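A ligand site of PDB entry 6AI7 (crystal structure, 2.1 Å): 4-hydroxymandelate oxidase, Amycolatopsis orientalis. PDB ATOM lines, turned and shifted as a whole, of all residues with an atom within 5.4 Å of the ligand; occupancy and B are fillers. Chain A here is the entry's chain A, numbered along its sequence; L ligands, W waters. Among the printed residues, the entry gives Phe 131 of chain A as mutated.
O4 of the ligand lies within hydrogen-bond range of N of Gly 309, at 3.1 Å.
O9 of the ligand lies within hydrogen-bond range of O of Pro 80 (2.8 Å).
OD2 of Asp 286 lies within hydrogen-bond range of O8 of the ligand (2.6 Å).
NH1 of Arg 310 lies within salt-bridge range of O6 of the ligand.
The backbone NH of Arg 310 sits at hydrogen-bond distance from an oxygen (O5) of the ligand.
O9 of the ligand sits at hydrogen-bond distance from NZ of Lys 231 (2.9 Å).
The side-chain hydroxyl (OG1) of Thr 157 lies within hydrogen-bond range of an oxygen (O1) of the ligand.
An oxygen (O6) of the ligand lies within salt-bridge range of the guanidinium group (NH2) of Arg 290, 2.7 Å away.
An oxygen (O6) of the ligand is in hydrogen-bond range of the backbone NH (N) of Gly 288, at 2.9 Å.
NE2 of His 255 is in hydrogen-bond range of O10 of the ligand, 2.8 Å away.
N of Ala 82 is in hydrogen-bond range of SG of Cys 109, at 3.7 Å.
A ring nitrogen (ND1) of His 255 is in hydrogen-bond range of the side-chain carboxylate (OD1) of Asp 159, at 2.8 Å.
The guanidinium group (NH1) of Arg 258 lies within hydrogen-bond range of the backbone carbonyl oxygen (O) of Phe 27 (3.0 Å).
The backbone carbonyl oxygen of Gly 256 sits at hydrogen-bond distance from the guanidinium group of Arg 310 (2.9 Å).
The backbone NH (N) of Phe 131 sits close to the side-chain amide nitrogen (NE2) of Gln 129.
The backbone NH of His 255 is in hydrogen-bond range of the side-chain hydroxyl of Ser 253, 2.9 Å away.
NE of Arg 310 sits at hydrogen-bond distance from O of Leu 28 (2.9 Å).
OG1 of Thr 157 sits close to NE2 of Gln 129 (3.2 Å).
O of Phe 27 touches C1 of the ligand, 3.5 Å away.
Leu 28 touches the ligand (O to C8, 3.4 Å).
CB of Ala 79 touches O9 of the ligand (3.8 Å).
Val 81 touches the ligand (CG1 to C2, 3.9 Å).
Ala 82 touches the ligand.
CD of Gln 129 touches N3 of the ligand (3.7 Å).
Phe 131 touches the ligand.
Ser 253 touches the ligand.
Gly 256 touches the ligand (N to O8, 3.9 Å).
Arg 258 touches the ligand (NH2 to C2, 3.5 Å).
CA of Gly 287 touches O3 of the ligand (3.5 Å).
Hydrophobic or aromatic side chains within 4 Å of the ligand: Phe 27, Leu 28, Ala 79, Pro 80, Val 81, Ala 82, Phe 131 and His 255.
20 residues have an atom within 4 Å of the ligand: Phe 27, Leu 28, Ala 79, Pro 80, Val 81, Ala 82, Gln 129, Phe 131, Thr 157, Lys 231, Ser 253, His 255, Gly 256, Arg 258, Asp 286, Gly 287, Gly 288, Arg 290, Gly 309 and Arg 310.
The nearest printed residue that does not touch the ligand is Val 308 (4.1 Å).
Water W3 lies within hydrogen-bond range of an oxygen (O6) of the ligand, the guanidinium group (NH1) of Arg 310 and the backbone carbonyl oxygen (O) of Gly 256.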
ATOM      1  N   PHE A  27     -29.160   7.240  -1.151  1.00  0.00           N
ATOM      2  CA  PHE A  27     -29.858   6.173  -1.833  1.00  0.00           C
ATOM      3  C   PHE A  27     -28.989   5.660  -3.002  1.00  0.00           C
ATOM      4  O   PHE A  27     -28.978   4.444  -3.298  1.00  0.00           O
ATOM      5  CB  PHE A  27     -31.197   6.649  -2.348  1.00  0.00           C
ATOM      6  CG  PHE A  27     -31.922   5.658  -3.224  1.00  0.00           C
ATOM      7  CD1 PHE A  27     -32.580   4.555  -2.669  1.00  0.00           C
ATOM      8  CD2 PHE A  27     -32.009   5.865  -4.598  1.00  0.00           C
ATOM      9  CE1 PHE A  27     -33.284   3.666  -3.489  1.00  0.00           C
ATOM     10  CE2 PHE A  27     -32.715   4.986  -5.415  1.00  0.00           C
ATOM     11  CZ  PHE A  27     -33.354   3.884  -4.856  1.00  0.00           C
ATOM     12  N   LEU A  28     -28.275   6.578  -3.642  1.00  0.00           N
ATOM     13  CA  LEU A  28     -27.440   6.242  -4.779  1.00  0.00           C
ATOM     14  C   LEU A  28     -26.116   5.580  -4.352  1.00  0.00           C
ATOM     15  O   LEU A  28     -25.716   4.530  -4.892  1.00  0.00           O
ATOM     16  CB  LEU A  28     -27.150   7.508  -5.599  1.00  0.00           C
ATOM     17  CG  LEU A  28     -26.331   7.337  -6.870  1.00  0.00           C
ATOM     18  CD1 LEU A  28     -26.818   6.162  -7.720  1.00  0.00           C
ATOM     19  CD2 LEU A  28     -26.376   8.636  -7.672  1.00  0.00           C
ATOM     20  N   ALA A  79     -25.837  -0.078 -16.327  1.00  0.00           N
ATOM     21  CA  ALA A  79     -26.381  -1.014 -15.380  1.00  0.00           C
ATOM     22  C   ALA A  79     -27.795  -0.610 -15.053  1.00  0.00           C
ATOM     23  O   ALA A  79     -28.083   0.549 -15.115  1.00  0.00           O
ATOM     24  CB  ALA A  79     -25.532  -1.051 -14.082  1.00  0.00           C
ATOM     25  N   PRO A  80     -28.648  -1.572 -14.653  1.00  0.00           N
ATOM     26  CA  PRO A  80     -29.952  -1.142 -14.229  1.00  0.00           C
ATOM     27  C   PRO A  80     -29.896  -0.428 -12.910  1.00  0.00           C
ATOM     28  O   PRO A  80     -29.299  -0.942 -11.902  1.00  0.00           O
ATOM     29  CB  PRO A  80     -30.741  -2.471 -14.062  1.00  0.00           C
ATOM     30  CG  PRO A  80     -29.663  -3.524 -13.802  1.00  0.00           C
ATOM     31  CD  PRO A  80     -28.514  -3.050 -14.647  1.00  0.00           C
ATOM     32  N   VAL A  81     -30.512   0.740 -12.886  1.00  0.00           N
ATOM     33  CA  VAL A  81     -30.636   1.573 -11.683  1.00  0.00           C
ATOM     34  C   VAL A  81     -32.043   2.131 -11.686  1.00  0.00           C
ATOM     35  O   VAL A  81     -32.459   2.693 -12.652  1.00  0.00           O
ATOM     36  CB  VAL A  81     -29.638   2.721 -11.699  1.00  0.00           C
ATOM     37  CG1 VAL A  81     -29.925   3.729 -10.577  1.00  0.00           C
ATOM     38  CG2 VAL A  81     -28.236   2.180 -11.537  1.00  0.00           C
ATOM     39  N   ALA A  82     -32.805   1.876 -10.639  1.00  0.00           N
ATOM     40  CA  ALA A  82     -34.198   2.317 -10.610  1.00  0.00           C
ATOM     41  C   ALA A  82     -34.435   3.820 -10.439  1.00  0.00           C
ATOM     42  O   ALA A  82     -33.613   4.543  -9.848  1.00  0.00           O
ATOM     43  CB  ALA A  82     -34.901   1.595  -9.498  1.00  0.00           C
ATOM     44  N   PHE A  87     -32.746  11.481 -10.186  1.00  0.00           N
ATOM     45  CA  PHE A  87     -31.456  12.181 -10.403  1.00  0.00           C
ATOM     46  C   PHE A  87     -31.520  13.342 -11.395  1.00  0.00           C
ATOM     47  O   PHE A  87     -30.651  14.238 -11.371  1.00  0.00           O
ATOM     48  CB  PHE A  87     -30.342  11.195 -10.809  1.00  0.00           C
ATOM     49  CG  PHE A  87     -30.385   9.910 -10.029  1.00  0.00           C
ATOM     50  CD1 PHE A  87     -30.073   9.904  -8.686  1.00  0.00           C
ATOM     51  CD2 PHE A  87     -30.836   8.733 -10.622  1.00  0.00           C
ATOM     52  CE1 PHE A  87     -30.163   8.739  -7.932  1.00  0.00           C
ATOM     53  CE2 PHE A  87     -30.901   7.555  -9.880  1.00  0.00           C
ATOM     54  CZ  PHE A  87     -30.570   7.564  -8.538  1.00  0.00           C
ATOM     55  N   CYS A 109     -34.736  -0.746 -16.204  1.00  0.00           N
ATOM     56  CA  CYS A 109     -35.248  -1.360 -14.970  1.00  0.00           C
ATOM     57  C   CYS A 109     -36.720  -1.616 -14.904  1.00  0.00           C
ATOM     58  O   CYS A 109     -37.547  -0.846 -15.481  1.00  0.00           O
ATOM     59  CB  CYS A 109     -35.011  -0.462 -13.805  1.00  0.00           C
ATOM     60  SG  CYS A 109     -33.289  -0.198 -13.658  1.00  0.00           S
ATOM     61  N   LEU A 111     -38.280  -1.139 -12.163  1.00  0.00           N
ATOM     62  CA  LEU A 111     -38.718   0.056 -11.507  1.00  0.00           C
ATOM     63  C   LEU A 111     -38.213   1.373 -12.157  1.00  0.00           C
ATOM     64  O   LEU A 111     -37.674   2.285 -11.478  1.00  0.00           O
ATOM     65  CB  LEU A 111     -38.214  -0.026 -10.072  1.00  0.00           C
ATOM     66  CG  LEU A 111     -38.682  -1.234  -9.262  1.00  0.00           C
ATOM     67  CD1 LEU A 111     -38.108  -1.111  -7.853  1.00  0.00           C
ATOM     68  CD2 LEU A 111     -40.203  -1.306  -9.187  1.00  0.00           C
ATOM     69  N   GLN A 129     -34.160  -5.371 -17.411  1.00  0.00           N
ATOM     70  CA  GLN A 129     -33.959  -5.993 -16.148  1.00  0.00           C
ATOM     71  C   GLN A 129     -35.307  -6.338 -15.484  1.00  0.00           C
ATOM     72  O   GLN A 129     -36.131  -5.456 -15.186  1.00  0.00           O
ATOM     73  CB  GLN A 129     -33.104  -5.127 -15.254  1.00  0.00           C
ATOM     74  CG  GLN A 129     -32.910  -5.671 -13.852  1.00  0.00           C
ATOM     75  CD  GLN A 129     -33.958  -5.140 -12.905  1.00  0.00           C
ATOM     76  OE1 GLN A 129     -34.372  -3.948 -12.967  1.00  0.00           O
ATOM     77  NE2 GLN A 129     -34.444  -6.020 -12.056  1.00  0.00           N
ATOM     78  N   PHE A 131     -37.327  -7.976 -12.248  1.00  0.00           N
ATOM     79  CA  PHE A 131     -37.548  -8.521 -10.922  1.00  0.00           C
ATOM     80  C   PHE A 131     -38.726  -9.431 -10.932  1.00  0.00           C
ATOM     81  O   PHE A 131     -39.741  -9.124 -11.541  1.00  0.00           O
ATOM     82  CB  PHE A 131     -37.904  -7.473  -9.971  1.00  0.00           C
ATOM     83  CG  PHE A 131     -36.790  -6.656  -9.530  1.00  0.00           C
ATOM     84  CD1 PHE A 131     -35.706  -7.231  -8.893  1.00  0.00           C
ATOM     85  CD2 PHE A 131     -36.874  -5.257  -9.590  1.00  0.00           C
ATOM     86  CE1 PHE A 131     -34.684  -6.450  -8.396  1.00  0.00           C
ATOM     87  CE2 PHE A 131     -35.836  -4.461  -9.127  1.00  0.00           C
ATOM     88  CZ  PHE A 131     -34.730  -5.061  -8.530  1.00  0.00           C
ATOM     89  N   THR A 157     -32.624 -10.336 -12.553  1.00  0.00           N
ATOM     90  CA  THR A 157     -31.893 -10.076 -11.355  1.00  0.00           C
ATOM     91  C   THR A 157     -32.295 -11.140 -10.345  1.00  0.00           C
ATOM     92  O   THR A 157     -33.467 -11.318 -10.085  1.00  0.00           O
ATOM     93  CB  THR A 157     -32.170  -8.688 -10.767  1.00  0.00           C
ATOM     94  OG1 THR A 157     -31.765  -7.716 -11.704  1.00  0.00           O
ATOM     95  CG2 THR A 157     -31.313  -8.438  -9.485  1.00  0.00           C
ATOM     96  N   ASP A 159     -30.434 -11.850  -7.383  1.00  0.00           N
ATOM     97  CA  ASP A 159     -29.834 -11.677  -6.069  1.00  0.00           C
ATOM     98  C   ASP A 159     -30.748 -10.804  -5.170  1.00  0.00           C
ATOM     99  O   ASP A 159     -30.332 -10.282  -4.100  1.00  0.00           O
ATOM    100  CB  ASP A 159     -28.347 -11.189  -6.116  1.00  0.00           C
ATOM    101  CG  ASP A 159     -28.183  -9.789  -6.741  1.00  0.00           C
ATOM    102  OD1 ASP A 159     -29.178  -9.232  -7.314  1.00  0.00           O
ATOM    103  OD2 ASP A 159     -27.067  -9.253  -6.619  1.00  0.00           O
ATOM    104  N   MET A 163     -35.006  -7.052  -0.825  1.00  0.00           N
ATOM    105  CA  MET A 163     -33.958  -6.025  -0.782  1.00  0.00           C
ATOM    106  C   MET A 163     -33.145  -6.167   0.490  1.00  0.00           C
ATOM    107  O   MET A 163     -33.704  -6.368   1.574  1.00  0.00           O
ATOM    108  CB  MET A 163     -34.571  -4.607  -0.877  1.00  0.00           C
ATOM    109  CG  MET A 163     -35.396  -4.352  -2.138  1.00  0.00           C
ATOM    110  SD  MET A 163     -34.538  -3.310  -3.346  1.00  0.00           S
ATOM    111  CE  MET A 163     -33.165  -4.342  -3.832  1.00  0.00           C
ATOM    112  N   LYS A 231     -28.358 -12.006 -13.264  1.00  0.00           N
ATOM    113  CA  LYS A 231     -27.512 -10.988 -12.672  1.00  0.00           C
ATOM    114  C   LYS A 231     -27.488 -11.119 -11.181  1.00  0.00           C
ATOM    115  O   LYS A 231     -28.535 -11.160 -10.559  1.00  0.00           O
ATOM    116  CB  LYS A 231     -27.974  -9.553 -13.038  1.00  0.00           C
ATOM    117  CG  LYS A 231     -27.325  -8.445 -12.195  1.00  0.00           C
ATOM    118  CD  LYS A 231     -27.692  -7.063 -12.784  1.00  0.00           C
ATOM    119  CE  LYS A 231     -26.926  -5.951 -12.103  1.00  0.00           C
ATOM    120  NZ  LYS A 231     -27.377  -5.706 -10.713  1.00  0.00           N
ATOM    121  N   SER A 253     -21.738 -10.380  -9.823  1.00  0.00           N
ATOM    122  CA  SER A 253     -22.020  -9.137  -9.196  1.00  0.00           C
ATOM    123  C   SER A 253     -22.505  -9.304  -7.757  1.00  0.00           C
ATOM    124  O   SER A 253     -23.225 -10.242  -7.508  1.00  0.00           O
ATOM    125  CB  SER A 253     -23.161  -8.540 -10.008  1.00  0.00           C
ATOM    126  OG  SER A 253     -23.773  -7.461  -9.353  1.00  0.00           O
ATOM    127  N   HIS A 255     -24.234  -6.898  -6.507  1.00  0.00           N
ATOM    128  CA  HIS A 255     -25.267  -5.885  -6.578  1.00  0.00           C
ATOM    129  C   HIS A 255     -24.728  -4.567  -5.977  1.00  0.00           C
ATOM    130  O   HIS A 255     -25.369  -3.896  -5.163  1.00  0.00           O
ATOM    131  CB  HIS A 255     -26.499  -6.462  -5.876  1.00  0.00           C
ATOM    132  CG  HIS A 255     -27.805  -5.822  -6.232  1.00  0.00           C
ATOM    133  ND1 HIS A 255     -28.808  -6.504  -6.905  1.00  0.00           N
ATOM    134  CD2 HIS A 255     -28.346  -4.608  -5.914  1.00  0.00           C
ATOM    135  CE1 HIS A 255     -29.868  -5.720  -7.039  1.00  0.00           C
ATOM    136  NE2 HIS A 255     -29.609  -4.575  -6.449  1.00  0.00           N
ATOM    137  N   GLY A 256     -23.506  -4.217  -6.302  1.00  0.00           N
ATOM    138  CA  GLY A 256     -22.911  -2.989  -5.782  1.00  0.00           C
ATOM    139  C   GLY A 256     -22.738  -2.887  -4.269  1.00  0.00           C
ATOM    140  O   GLY A 256     -22.625  -1.773  -3.752  1.00  0.00           O
ATOM    141  N   ARG A 258     -25.005  -3.881  -2.143  1.00  0.00           N
ATOM    142  CA  ARG A 258     -26.350  -3.415  -1.691  1.00  0.00           C
ATOM    143  C   ARG A 258     -27.230  -4.573  -1.178  1.00  0.00           C
ATOM    144  O   ARG A 258     -28.370  -4.348  -0.620  1.00  0.00           O
ATOM    145  CB  ARG A 258     -27.091  -2.656  -2.846  1.00  0.00           C
ATOM    146  CG  ARG A 258     -26.390  -1.380  -3.292  1.00  0.00           C
ATOM    147  CD  ARG A 258     -26.945  -0.767  -4.580  1.00  0.00           C
ATOM    148  NE  ARG A 258     -28.310  -0.266  -4.467  1.00  0.00           N
ATOM    149  CZ  ARG A 258     -28.656   0.899  -3.893  1.00  0.00           C
ATOM    150  NH1 ARG A 258     -27.751   1.692  -3.336  1.00  0.00           N
ATOM    151  NH2 ARG A 258     -29.935   1.233  -3.875  1.00  0.00           N
ATOM    152  N   ASP A 286     -19.787  -6.511 -12.644  1.00  0.00           N
ATOM    153  CA  ASP A 286     -19.897  -5.120 -12.254  1.00  0.00           C
ATOM    154  C   ASP A 286     -19.450  -4.921 -10.816  1.00  0.00           C
ATOM    155  O   ASP A 286     -19.019  -5.887 -10.127  1.00  0.00           O
ATOM    156  CB  ASP A 286     -21.289  -4.600 -12.499  1.00  0.00           C
ATOM    157  CG  ASP A 286     -22.343  -5.168 -11.531  1.00  0.00           C
ATOM    158  OD1 ASP A 286     -21.995  -5.718 -10.453  1.00  0.00           O
ATOM    159  OD2 ASP A 286     -23.563  -4.975 -11.864  1.00  0.00           O
ATOM    160  N   GLY A 287     -19.536  -3.672 -10.380  1.00  0.00           N
ATOM    161  CA  GLY A 287     -19.144  -3.282  -9.050  1.00  0.00           C
ATOM    162  C   GLY A 287     -17.843  -2.511  -9.073  1.00  0.00           C
ATOM    163  O   GLY A 287     -16.742  -3.078  -9.217  1.00  0.00           O
ATOM    164  N   GLY A 288     -17.965  -1.201  -8.968  1.00  0.00           N
ATOM    165  CA  GLY A 288     -16.817  -0.355  -8.793  1.00  0.00           C
ATOM    166  C   GLY A 288     -16.036  -0.001 -10.016  1.00  0.00           C
ATOM    167  O   GLY A 288     -14.907   0.435  -9.909  1.00  0.00           O
ATOM    168  N   ILE A 289     -16.574  -0.264 -11.201  1.00  0.00           N
ATOM    169  CA  ILE A 289     -15.854   0.030 -12.404  1.00  0.00           C
ATOM    170  C   ILE A 289     -15.885   1.570 -12.529  1.00  0.00           C
ATOM    171  O   ILE A 289     -16.965   2.153 -12.627  1.00  0.00           O
ATOM    172  CB  ILE A 289     -16.492  -0.600 -13.634  1.00  0.00           C
ATOM    173  CG1 ILE A 289     -16.563  -2.121 -13.519  1.00  0.00           C
ATOM    174  CG2 ILE A 289     -15.770  -0.169 -14.858  1.00  0.00           C
ATOM    175  CD1 ILE A 289     -15.240  -2.900 -13.510  1.00  0.00           C
ATOM    176  N   ARG A 290     -14.706   2.203 -12.499  1.00  0.00           N
ATOM    177  CA  ARG A 290     -14.571   3.686 -12.420  1.00  0.00           C
ATOM    178  C   ARG A 290     -13.634   4.299 -13.478  1.00  0.00           C
ATOM    179  O   ARG A 290     -13.318   5.465 -13.394  1.00  0.00           O
ATOM    180  CB  ARG A 290     -14.105   4.125 -10.981  1.00  0.00           C
ATOM    181  CG  ARG A 290     -15.080   3.817  -9.831  1.00  0.00           C
ATOM    182  CD  ARG A 290     -16.477   4.417 -10.034  1.00  0.00           C
ATOM    183  NE  ARG A 290     -17.459   3.997  -8.994  1.00  0.00           N
ATOM    184  CZ  ARG A 290     -18.362   3.022  -9.110  1.00  0.00           C
ATOM    185  NH1 ARG A 290     -18.474   2.257 -10.199  1.00  0.00           N
ATOM    186  NH2 ARG A 290     -19.191   2.799  -8.095  1.00  0.00           N
ATOM    187  N   LEU A 307     -20.712  -3.829 -16.431  1.00  0.00           N
ATOM    188  CA  LEU A 307     -21.818  -2.875 -16.287  1.00  0.00           C
ATOM    189  C   LEU A 307     -21.292  -1.727 -15.462  1.00  0.00           C
ATOM    190  O   LEU A 307     -20.407  -1.903 -14.595  1.00  0.00           O
ATOM    191  CB  LEU A 307     -22.997  -3.470 -15.539  1.00  0.00           C
ATOM    192  CG  LEU A 307     -23.594  -4.724 -16.135  1.00  0.00           C
ATOM    193  CD1 LEU A 307     -24.844  -5.006 -15.331  1.00  0.00           C
ATOM    194  CD2 LEU A 307     -23.944  -4.566 -17.556  1.00  0.00           C
ATOM    195  N   VAL A 308     -21.825  -0.547 -15.724  1.00  0.00           N
ATOM    196  CA  VAL A 308     -21.510   0.683 -14.960  1.00  0.00           C
ATOM    197  C   VAL A 308     -22.803   1.297 -14.473  1.00  0.00           C
ATOM    198  O   VAL A 308     -23.733   1.498 -15.283  1.00  0.00           O
ATOM    199  CB  VAL A 308     -20.705   1.701 -15.772  1.00  0.00           C
ATOM    200  CG1 VAL A 308     -20.238   2.827 -14.857  1.00  0.00           C
ATOM    201  CG2 VAL A 308     -19.490   1.036 -16.392  1.00  0.00           C
ATOM    202  N   GLY A 309     -22.884   1.478 -13.149  1.00  0.00           N
ATOM    203  CA  GLY A 309     -24.073   1.931 -12.467  1.00  0.00           C
ATOM    204  C   GLY A 309     -23.934   3.361 -11.917  1.00  0.00           C
ATOM    205  O   GLY A 309     -24.230   4.304 -12.601  1.00  0.00           O
ATOM    206  N   ARG A 310     -23.412   3.513 -10.703  1.00  0.00           N
ATOM    207  CA  ARG A 310     -23.479   4.818 -10.055  1.00  0.00           C
ATOM    208  C   ARG A 310     -22.865   5.925 -10.878  1.00  0.00           C
ATOM    209  O   ARG A 310     -23.483   6.998 -10.947  1.00  0.00           O
ATOM    210  CB  ARG A 310     -22.878   4.813  -8.669  1.00  0.00           C
ATOM    211  CG  ARG A 310     -23.632   3.975  -7.645  1.00  0.00           C
ATOM    212  CD  ARG A 310     -22.730   3.783  -6.432  1.00  0.00           C
ATOM    213  NE  ARG A 310     -23.339   2.915  -5.404  1.00  0.00           N
ATOM    214  CZ  ARG A 310     -23.026   1.626  -5.214  1.00  0.00           C
ATOM    215  NH1 ARG A 310     -22.109   1.001  -5.993  1.00  0.00           N
ATOM    216  NH2 ARG A 310     -23.635   0.953  -4.218  1.00  0.00           N
ATOM    217  N   PRO A 311     -21.713   5.663 -11.567  1.00  0.00           N
ATOM    218  CA  PRO A 311     -21.190   6.756 -12.391  1.00  0.00           C
ATOM    219  C   PRO A 311     -22.105   7.309 -13.420  1.00  0.00           C
ATOM    220  O   PRO A 311     -21.975   8.464 -13.745  1.00  0.00           O
ATOM    221  CB  PRO A 311     -19.954   6.174 -13.051  1.00  0.00           C
ATOM    222  CG  PRO A 311     -19.504   5.066 -12.110  1.00  0.00           C
ATOM    223  CD  PRO A 311     -20.674   4.655 -11.243  1.00  0.00           C
HETATM  224  C1  LIG L   1     -29.330   3.407  -6.644  1.00  0.00           C
HETATM  225  C2  LIG L   1     -29.128   2.111  -7.166  1.00  0.00           C
HETATM  226  C3  LIG L   1     -30.253   1.296  -7.412  1.00  0.00           C
HETATM  227  C4  LIG L   1     -30.056   0.016  -7.917  1.00  0.00           C
HETATM  228  C5  LIG L   1     -28.784  -0.527  -8.194  1.00  0.00           C
HETATM  229  C6  LIG L   1     -27.709   0.331  -7.973  1.00  0.00           C
HETATM  230  C7  LIG L   1     -27.848   1.617  -7.455  1.00  0.00           C
HETATM  231  C8  LIG L   1     -26.640   2.325  -7.258  1.00  0.00           C
HETATM  232  C9  LIG L   1     -29.686  -2.462  -9.226  1.00  0.00           C
HETATM  233  C10 LIG L   1     -30.610  -4.380 -10.255  1.00  0.00           C
HETATM  234  C11 LIG L   1     -32.033  -2.401  -9.610  1.00  0.00           C
HETATM  235  C12 LIG L   1     -30.970  -1.958  -8.879  1.00  0.00           C
HETATM  236  C13 LIG L   1     -27.248  -2.482  -8.853  1.00  0.00           C
HETATM  237  C14 LIG L   1     -26.624  -2.198 -10.219  1.00  0.00           C
HETATM  238  C15 LIG L   1     -25.145  -2.670 -10.299  1.00  0.00           C
HETATM  239  C16 LIG L   1     -24.206  -1.872  -9.385  1.00  0.00           C
HETATM  240  C17 LIG L   1     -22.853  -1.824 -10.089  1.00  0.00           C
HETATM  241  N1  LIG L   1     -28.613  -1.803  -8.724  1.00  0.00           N
HETATM  242  N2  LIG L   1     -29.524  -3.713  -9.769  1.00  0.00           N
HETATM  243  N3  LIG L   1     -31.884  -3.704 -10.165  1.00  0.00           N
HETATM  244  N4  LIG L   1     -31.137  -0.703  -8.171  1.00  0.00           N
HETATM  245  O1  LIG L   1     -30.515  -5.534 -10.772  1.00  0.00           O
HETATM  246  O2  LIG L   1     -33.160  -1.868  -9.474  1.00  0.00           O
HETATM  247  O3  LIG L   1     -22.006  -1.271  -9.169  1.00  0.00           O
HETATM  248  O4  LIG L   1     -20.981   0.520 -10.933  1.00  0.00           O
HETATM  249  O5  LIG L   1     -22.753   1.231  -9.196  1.00  0.00           O
HETATM  250  O6  LIG L   1     -20.325   0.413  -8.443  1.00  0.00           O
HETATM  251  O7  LIG L   1     -24.632  -0.470  -9.201  1.00  0.00           O
HETATM  252  O8  LIG L   1     -25.006  -4.046  -9.893  1.00  0.00           O
HETATM  253  O9  LIG L   1     -27.315  -2.852 -11.293  1.00  0.00           O
HETATM  254  O10 LIG L   1     -31.267  -2.644  -7.612  1.00  0.00           O
HETATM  255  P1  LIG L   1     -21.431   0.233  -9.416  1.00  0.00           P
HETATM  256  O   HOH W   1     -19.475  -1.284 -11.985  1.00  0.00           O
HETATM  257  O   HOH W   2     -33.477  -1.640  -6.767  1.00  0.00           O
HETATM  258  O   HOH W   3     -19.965  -1.175  -5.908  1.00  0.00           O
